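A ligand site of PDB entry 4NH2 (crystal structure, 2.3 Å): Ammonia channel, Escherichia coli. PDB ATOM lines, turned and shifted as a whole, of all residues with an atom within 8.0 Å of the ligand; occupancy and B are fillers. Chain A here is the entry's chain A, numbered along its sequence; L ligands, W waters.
O9 of the ligand lies within hydrogen-bond range of ND2 of Asn 72, 2.7 Å away.
N of Ile 78 sits at hydrogen-bond distance from O8 of the ligand.
Residues that only touch the ligand: Phe 75 (3.4 Å), Gly 76 (3.1 Å), Asn 77 (3.4 Å) and Asn 79 (3.6 Å).
Hydrophobic or aromatic side chains that line the ligand: Phe 75 and Ile 78.
Of the 21 residues printed, 6 come within 4 Å of the ligand.
Water W1 lies within hydrogen-bond range of ND2 of Asn 79, O8 of the ligand and N of Ile 78.
OD1 of Asn 72 is in hydrogen-bond range of N of Phe 75, at 3.0 Å.
OD1 of Asn 72 sits at hydrogen-bond distance from N of Phe 74, 2.8 Å away.
O of Asn 72 lies within hydrogen-bond range of NE2 of His 145 (2.9 Å).
The backbone NH (N) of Gly 76 lies within hydrogen-bond range of the backbone carbonyl oxygen (O) of Leu 66, at 2.7 Å.
O of Phe 75 sits at hydrogen-bond distance from NE2 of His 145 (3.2 Å).
The backbone NH (N) of Asn 79 lies within hydrogen-bond range of the side-chain amide oxygen (OD1) of Asn 77, 3.0 Å away.
ND2 of Asn 77 lies within hydrogen-bond range of O of Glu 70, at 2.8 Å.
The backbone carbonyl oxygen of Asn 77 lies within hydrogen-bond range of the backbone NH of Leu 66 (3.2 Å).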
ATOM      1  N   TYR A  62       7.291 -13.773 -10.191  1.00  0.00           N
ATOM      2  CA  TYR A  62       8.512 -14.503  -9.730  1.00  0.00           C
ATOM      3  C   TYR A  62       9.400 -15.052 -10.835  1.00  0.00           C
ATOM      4  O   TYR A  62      10.564 -15.355 -10.595  1.00  0.00           O
ATOM      5  CB  TYR A  62       8.140 -15.688  -8.769  1.00  0.00           C
ATOM      6  CG  TYR A  62       7.381 -16.845  -9.388  1.00  0.00           C
ATOM      7  CD1 TYR A  62       8.048 -17.906  -9.931  1.00  0.00           C
ATOM      8  CD2 TYR A  62       5.968 -16.861  -9.404  1.00  0.00           C
ATOM      9  CE1 TYR A  62       7.364 -18.911 -10.552  1.00  0.00           C
ATOM     10  CE2 TYR A  62       5.258 -17.886  -9.988  1.00  0.00           C
ATOM     11  CZ  TYR A  62       5.965 -18.906 -10.578  1.00  0.00           C
ATOM     12  OH  TYR A  62       5.316 -19.920 -11.207  1.00  0.00           O
ATOM     13  N   SER A  65      12.829 -13.455 -12.010  1.00  0.00           N
ATOM     14  CA  SER A  65      13.777 -13.555 -10.889  1.00  0.00           C
ATOM     15  C   SER A  65      14.353 -14.960 -10.754  1.00  0.00           C
ATOM     16  O   SER A  65      15.557 -15.146 -10.560  1.00  0.00           O
ATOM     17  CB  SER A  65      13.025 -13.158  -9.602  1.00  0.00           C
ATOM     18  OG  SER A  65      13.815 -13.217  -8.446  1.00  0.00           O
ATOM     19  N   LEU A  66      13.490 -15.958 -10.896  1.00  0.00           N
ATOM     20  CA  LEU A  66      13.902 -17.333 -10.721  1.00  0.00           C
ATOM     21  C   LEU A  66      14.680 -17.831 -11.895  1.00  0.00           C
ATOM     22  O   LEU A  66      15.437 -18.827 -11.805  1.00  0.00           O
ATOM     23  CB  LEU A  66      12.634 -18.197 -10.457  1.00  0.00           C
ATOM     24  CG  LEU A  66      12.859 -19.573  -9.868  1.00  0.00           C
ATOM     25  CD1 LEU A  66      13.617 -19.507  -8.557  1.00  0.00           C
ATOM     26  CD2 LEU A  66      11.500 -20.237  -9.660  1.00  0.00           C
ATOM     27  N   GLY A  69      17.890 -14.090 -11.831  1.00  0.00           N
ATOM     28  CA  GLY A  69      18.568 -13.651 -10.586  1.00  0.00           C
ATOM     29  C   GLY A  69      19.715 -14.569 -10.158  1.00  0.00           C
ATOM     30  O   GLY A  69      19.852 -15.693 -10.675  1.00  0.00           O
ATOM     31  N   GLU A  70      20.568 -14.100  -9.248  1.00  0.00           N
ATOM     32  CA  GLU A  70      21.630 -14.955  -8.715  1.00  0.00           C
ATOM     33  C   GLU A  70      21.053 -16.083  -7.921  1.00  0.00           C
ATOM     34  O   GLU A  70      20.135 -15.912  -7.117  1.00  0.00           O
ATOM     35  CB  GLU A  70      22.704 -14.228  -7.914  1.00  0.00           C
ATOM     36  CG  GLU A  70      24.143 -14.506  -8.422  1.00  0.00           C
ATOM     37  CD  GLU A  70      25.160 -14.425  -7.308  1.00  0.00           C
ATOM     38  OE1 GLU A  70      24.971 -13.552  -6.413  1.00  0.00           O
ATOM     39  OE2 GLU A  70      26.147 -15.223  -7.341  1.00  0.00           O
ATOM     40  N   GLY A  71      21.556 -17.264  -8.162  1.00  0.00           N
ATOM     41  CA  GLY A  71      21.077 -18.418  -7.438  1.00  0.00           C
ATOM     42  C   GLY A  71      22.159 -19.431  -7.365  1.00  0.00           C
ATOM     43  O   GLY A  71      23.278 -19.154  -6.927  1.00  0.00           O
ATOM     44  N   ASN A  72      21.858 -20.626  -7.808  1.00  0.00           N
ATOM     45  CA  ASN A  72      22.875 -21.673  -7.932  1.00  0.00           C
ATOM     46  C   ASN A  72      23.069 -21.992  -9.434  1.00  0.00           C
ATOM     47  O   ASN A  72      22.827 -21.150 -10.307  1.00  0.00           O
ATOM     48  CB  ASN A  72      22.513 -22.903  -7.049  1.00  0.00           C
ATOM     49  CG  ASN A  72      21.081 -23.446  -7.295  1.00  0.00           C
ATOM     50  OD1 ASN A  72      20.666 -23.735  -8.435  1.00  0.00           O
ATOM     51  ND2 ASN A  72      20.325 -23.591  -6.215  1.00  0.00           N
ATOM     52  N   ASN A  73      23.595 -23.161  -9.752  1.00  0.00           N
ATOM     53  CA  ASN A  73      23.729 -23.586 -11.141  1.00  0.00           C
ATOM     54  C   ASN A  73      22.395 -23.897 -11.851  1.00  0.00           C
ATOM     55  O   ASN A  73      22.372 -23.962 -13.082  1.00  0.00           O
ATOM     56  CB  ASN A  73      24.630 -24.815 -11.232  1.00  0.00           C
ATOM     57  CG  ASN A  73      26.125 -24.461 -11.207  1.00  0.00           C
ATOM     58  OD1 ASN A  73      26.612 -23.676 -12.015  1.00  0.00           O
ATOM     59  ND2 ASN A  73      26.862 -25.109 -10.308  1.00  0.00           N
ATOM     60  N   PHE A  74      21.300 -24.031 -11.102  1.00  0.00           N
ATOM     61  CA  PHE A  74      20.022 -24.449 -11.669  1.00  0.00           C
ATOM     62  C   PHE A  74      18.858 -23.432 -11.639  1.00  0.00           C
ATOM     63  O   PHE A  74      18.056 -23.372 -12.568  1.00  0.00           O
ATOM     64  CB  PHE A  74      19.603 -25.756 -11.023  1.00  0.00           C
ATOM     65  CG  PHE A  74      20.637 -26.840 -11.159  1.00  0.00           C
ATOM     66  CD1 PHE A  74      20.724 -27.564 -12.321  1.00  0.00           C
ATOM     67  CD2 PHE A  74      21.579 -27.078 -10.139  1.00  0.00           C
ATOM     68  CE1 PHE A  74      21.700 -28.534 -12.477  1.00  0.00           C
ATOM     69  CE2 PHE A  74      22.564 -28.049 -10.283  1.00  0.00           C
ATOM     70  CZ  PHE A  74      22.620 -28.777 -11.458  1.00  0.00           C
ATOM     71  N   PHE A  75      18.768 -22.665 -10.545  1.00  0.00           N
ATOM     72  CA  PHE A  75      17.710 -21.715 -10.339  1.00  0.00           C
ATOM     73  C   PHE A  75      18.290 -20.369  -9.861  1.00  0.00           C
ATOM     74  O   PHE A  75      19.403 -20.301  -9.331  1.00  0.00           O
ATOM     75  CB  PHE A  75      16.727 -22.228  -9.269  1.00  0.00           C
ATOM     76  CG  PHE A  75      15.845 -23.384  -9.703  1.00  0.00           C
ATOM     77  CD1 PHE A  75      16.276 -24.699  -9.585  1.00  0.00           C
ATOM     78  CD2 PHE A  75      14.548 -23.164 -10.143  1.00  0.00           C
ATOM     79  CE1 PHE A  75      15.444 -25.773  -9.933  1.00  0.00           C
ATOM     80  CE2 PHE A  75      13.711 -24.219 -10.479  1.00  0.00           C
ATOM     81  CZ  PHE A  75      14.160 -25.515 -10.409  1.00  0.00           C
ATOM     82  N   GLY A  76      17.516 -19.314 -10.079  1.00  0.00           N
ATOM     83  CA  GLY A  76      17.841 -17.951  -9.600  1.00  0.00           C
ATOM     84  C   GLY A  76      17.294 -17.817  -8.209  1.00  0.00           C
ATOM     85  O   GLY A  76      17.562 -18.639  -7.372  1.00  0.00           O
ATOM     86  N   ASN A  77      16.424 -16.855  -7.982  1.00  0.00           N
ATOM     87  CA  ASN A  77      15.883 -16.697  -6.683  1.00  0.00           C
ATOM     88  C   ASN A  77      14.507 -16.049  -6.796  1.00  0.00           C
ATOM     89  O   ASN A  77      14.158 -15.545  -7.845  1.00  0.00           O
ATOM     90  CB  ASN A  77      16.863 -15.829  -5.857  1.00  0.00           C
ATOM     91  CG  ASN A  77      16.911 -14.427  -6.373  1.00  0.00           C
ATOM     92  OD1 ASN A  77      16.014 -13.629  -6.083  1.00  0.00           O
ATOM     93  ND2 ASN A  77      17.952 -14.081  -7.101  1.00  0.00           N
ATOM     94  N   ILE A  78      13.780 -16.033  -5.685  1.00  0.00           N
ATOM     95  CA  ILE A  78      12.520 -15.328  -5.542  1.00  0.00           C
ATOM     96  C   ILE A  78      12.608 -14.484  -4.289  1.00  0.00           C
ATOM     97  O   ILE A  78      11.683 -14.471  -3.514  1.00  0.00           O
ATOM     98  CB  ILE A  78      11.290 -16.260  -5.419  1.00  0.00           C
ATOM     99  CG1 ILE A  78      11.406 -17.228  -4.227  1.00  0.00           C
ATOM    100  CG2 ILE A  78      11.116 -17.104  -6.679  1.00  0.00           C
ATOM    101  CD1 ILE A  78      10.148 -18.070  -3.961  1.00  0.00           C
ATOM    102  N   ASN A  79      13.718 -13.773  -4.107  1.00  0.00           N
ATOM    103  CA  ASN A  79      13.900 -12.887  -2.939  1.00  0.00           C
ATOM    104  C   ASN A  79      13.016 -11.668  -3.034  1.00  0.00           C
ATOM    105  O   ASN A  79      12.648 -11.078  -2.026  1.00  0.00           O
ATOM    106  CB  ASN A  79      15.352 -12.398  -2.812  1.00  0.00           C
ATOM    107  CG  ASN A  79      16.335 -13.493  -2.536  1.00  0.00           C
ATOM    108  OD1 ASN A  79      17.547 -13.356  -2.837  1.00  0.00           O
ATOM    109  ND2 ASN A  79      15.873 -14.581  -1.973  1.00  0.00           N
ATOM    110  N   TRP A  80      12.677 -11.283  -4.255  1.00  0.00           N
ATOM    111  CA  TRP A  80      11.823 -10.115  -4.503  1.00  0.00           C
ATOM    112  C   TRP A  80      10.731 -10.436  -5.554  1.00  0.00           C
ATOM    113  O   TRP A  80      10.987 -11.010  -6.629  1.00  0.00           O
ATOM    114  CB  TRP A  80      12.667  -8.962  -5.010  1.00  0.00           C
ATOM    115  CG  TRP A  80      13.924  -8.664  -4.209  1.00  0.00           C
ATOM    116  CD1 TRP A  80      15.164  -9.280  -4.330  1.00  0.00           C
ATOM    117  CD2 TRP A  80      14.082  -7.659  -3.225  1.00  0.00           C
ATOM    118  NE1 TRP A  80      16.085  -8.707  -3.452  1.00  0.00           N
ATOM    119  CE2 TRP A  80      15.444  -7.714  -2.753  1.00  0.00           C
ATOM    120  CE3 TRP A  80      13.196  -6.731  -2.637  1.00  0.00           C
ATOM    121  CZ2 TRP A  80      15.937  -6.862  -1.732  1.00  0.00           C
ATOM    122  CZ3 TRP A  80      13.700  -5.881  -1.642  1.00  0.00           C
ATOM    123  CH2 TRP A  80      15.058  -5.972  -1.193  1.00  0.00           C
ATOM    124  N   THR A 137       7.691 -23.212 -14.258  1.00  0.00           N
ATOM    125  CA  THR A 137       8.430 -22.992 -13.038  1.00  0.00           C
ATOM    126  C   THR A 137       9.618 -23.921 -12.893  1.00  0.00           C
ATOM    127  O   THR A 137      10.663 -23.518 -12.358  1.00  0.00           O
ATOM    128  CB  THR A 137       7.501 -23.143 -11.833  1.00  0.00           C
ATOM    129  OG1 THR A 137       6.307 -22.380 -12.061  1.00  0.00           O
ATOM    130  CG2 THR A 137       8.167 -22.691 -10.579  1.00  0.00           C
ATOM    131  N   LEU A 138       9.441 -25.176 -13.322  1.00  0.00           N
ATOM    132  CA  LEU A 138      10.420 -26.194 -13.008  1.00  0.00           C
ATOM    133  C   LEU A 138      11.164 -26.742 -14.201  1.00  0.00           C
ATOM    134  O   LEU A 138      12.143 -27.465 -14.018  1.00  0.00           O
ATOM    135  CB  LEU A 138       9.749 -27.327 -12.224  1.00  0.00           C
ATOM    136  CG  LEU A 138       9.212 -26.978 -10.814  1.00  0.00           C
ATOM    137  CD1 LEU A 138       8.527 -28.193 -10.177  1.00  0.00           C
ATOM    138  CD2 LEU A 138      10.342 -26.494  -9.922  1.00  0.00           C
ATOM    139  N   ILE A 141      12.123 -22.273 -16.603  1.00  0.00           N
ATOM    140  CA  ILE A 141      12.850 -21.325 -15.795  1.00  0.00           C
ATOM    141  C   ILE A 141      14.251 -21.777 -15.438  1.00  0.00           C
ATOM    142  O   ILE A 141      15.209 -21.029 -15.652  1.00  0.00           O
ATOM    143  CB  ILE A 141      12.003 -20.926 -14.597  1.00  0.00           C
ATOM    144  CG1 ILE A 141      10.997 -19.846 -15.084  1.00  0.00           C
ATOM    145  CG2 ILE A 141      12.877 -20.434 -13.424  1.00  0.00           C
ATOM    146  CD1 ILE A 141       9.834 -19.559 -14.120  1.00  0.00           C
ATOM    147  N   PRO A 142      14.398 -23.034 -14.993  1.00  0.00           N
ATOM    148  CA  PRO A 142      15.786 -23.440 -14.653  1.00  0.00           C
ATOM    149  C   PRO A 142      16.630 -23.683 -15.857  1.00  0.00           C
ATOM    150  O   PRO A 142      17.813 -23.357 -15.867  1.00  0.00           O
ATOM    151  CB  PRO A 142      15.587 -24.760 -13.861  1.00  0.00           C
ATOM    152  CG  PRO A 142      14.164 -25.219 -14.149  1.00  0.00           C
ATOM    153  CD  PRO A 142      13.375 -24.016 -14.556  1.00  0.00           C
ATOM    154  N   HIS A 145      17.857 -20.504 -16.819  1.00  0.00           N
ATOM    155  CA  HIS A 145      18.877 -20.072 -15.847  1.00  0.00           C
ATOM    156  C   HIS A 145      20.176 -20.727 -16.210  1.00  0.00           C
ATOM    157  O   HIS A 145      21.226 -20.056 -16.230  1.00  0.00           O
ATOM    158  CB  HIS A 145      18.523 -20.417 -14.394  1.00  0.00           C
ATOM    159  CG  HIS A 145      19.531 -19.885 -13.405  1.00  0.00           C
ATOM    160  ND1 HIS A 145      19.564 -18.559 -13.029  1.00  0.00           N
ATOM    161  CD2 HIS A 145      20.540 -20.486 -12.729  1.00  0.00           C
ATOM    162  CE1 HIS A 145      20.549 -18.362 -12.171  1.00  0.00           C
ATOM    163  NE2 HIS A 145      21.144 -19.526 -11.954  1.00  0.00           N
ATOM    164  N   TRP A 365      15.767 -33.522 -18.110  1.00  0.00           N
ATOM    165  CA  TRP A 365      15.106 -32.537 -17.248  1.00  0.00           C
ATOM    166  C   TRP A 365      13.631 -32.203 -17.630  1.00  0.00           C
ATOM    167  O   TRP A 365      12.799 -32.006 -16.766  1.00  0.00           O
ATOM    168  CB  TRP A 365      15.904 -31.229 -17.260  1.00  0.00           C
ATOM    169  CG  TRP A 365      15.536 -30.270 -16.157  1.00  0.00           C
ATOM    170  CD1 TRP A 365      14.382 -29.561 -16.029  1.00  0.00           C
ATOM    171  CD2 TRP A 365      16.373 -29.906 -15.052  1.00  0.00           C
ATOM    172  NE1 TRP A 365      14.439 -28.796 -14.884  1.00  0.00           N
ATOM    173  CE2 TRP A 365      15.648 -29.008 -14.267  1.00  0.00           C
ATOM    174  CE3 TRP A 365      17.663 -30.284 -14.642  1.00  0.00           C
ATOM    175  CZ2 TRP A 365      16.169 -28.458 -13.108  1.00  0.00           C
ATOM    176  CZ3 TRP A 365      18.166 -29.752 -13.505  1.00  0.00           C
ATOM    177  CH2 TRP A 365      17.426 -28.836 -12.743  1.00  0.00           C
HETATM  178  C1  LIG L   1      21.145 -17.431  -3.543  1.00  0.00           C
HETATM  179  C2  LIG L   1      21.428 -16.333  -2.518  1.00  0.00           C
HETATM  180  O1  LIG L   1      20.635 -15.182  -2.923  1.00  0.00           O
HETATM  181  O2  LIG L   1      15.392 -21.049  -4.672  1.00  0.00           O
HETATM  182  C3  LIG L   1      16.808 -20.924  -4.563  1.00  0.00           C
HETATM  183  C4  LIG L   1      17.188 -21.529  -5.867  1.00  0.00           C
HETATM  184  C5  LIG L   1      17.463 -19.552  -4.418  1.00  0.00           C
HETATM  185  O3  LIG L   1      17.629 -22.811  -5.538  1.00  0.00           O
HETATM  186  O4  LIG L   1      18.889 -19.620  -4.220  1.00  0.00           O
HETATM  187  O5  LIG L   1      18.569 -18.316  -2.052  1.00  0.00           O
HETATM  188  P1  LIG L   1      19.469 -19.363  -2.693  1.00  0.00           P
HETATM  189  O6  LIG L   1      20.937 -18.677  -2.893  1.00  0.00           O
HETATM  190  O7  LIG L   1      19.761 -20.691  -1.969  1.00  0.00           O
HETATM  191  C6  LIG L   1      14.503 -20.111  -4.125  1.00  0.00           C
HETATM  192  O8  LIG L   1      14.745 -18.932  -4.320  1.00  0.00           O
HETATM  193  C7  LIG L   1      17.065 -24.029  -6.089  1.00  0.00           C
HETATM  194  O9  LIG L   1      17.923 -24.890  -6.298  1.00  0.00           O
HETATM  195  C8  LIG L   1      13.239 -20.636  -3.428  1.00  0.00           C
HETATM  196  C9  LIG L   1      12.685 -21.950  -4.029  1.00  0.00           C
HETATM  197  C10 LIG L   1      11.624 -21.771  -5.129  1.00  0.00           C
HETATM  198  C11 LIG L   1      11.899 -22.750  -6.288  1.00  0.00           C
HETATM  199  C12 LIG L   1      15.574 -24.191  -6.337  1.00  0.00           C
HETATM  200  C13 LIG L   1      15.290 -25.694  -6.539  1.00  0.00           C
HETATM  201  C14 LIG L   1      22.949 -16.041  -2.414  1.00  0.00           C
HETATM  202  O10 LIG L   1      23.727 -17.139  -1.903  1.00  0.00           O
HETATM  203  O   HOH W   1      15.175 -16.751  -2.748  1.00  0.00           O
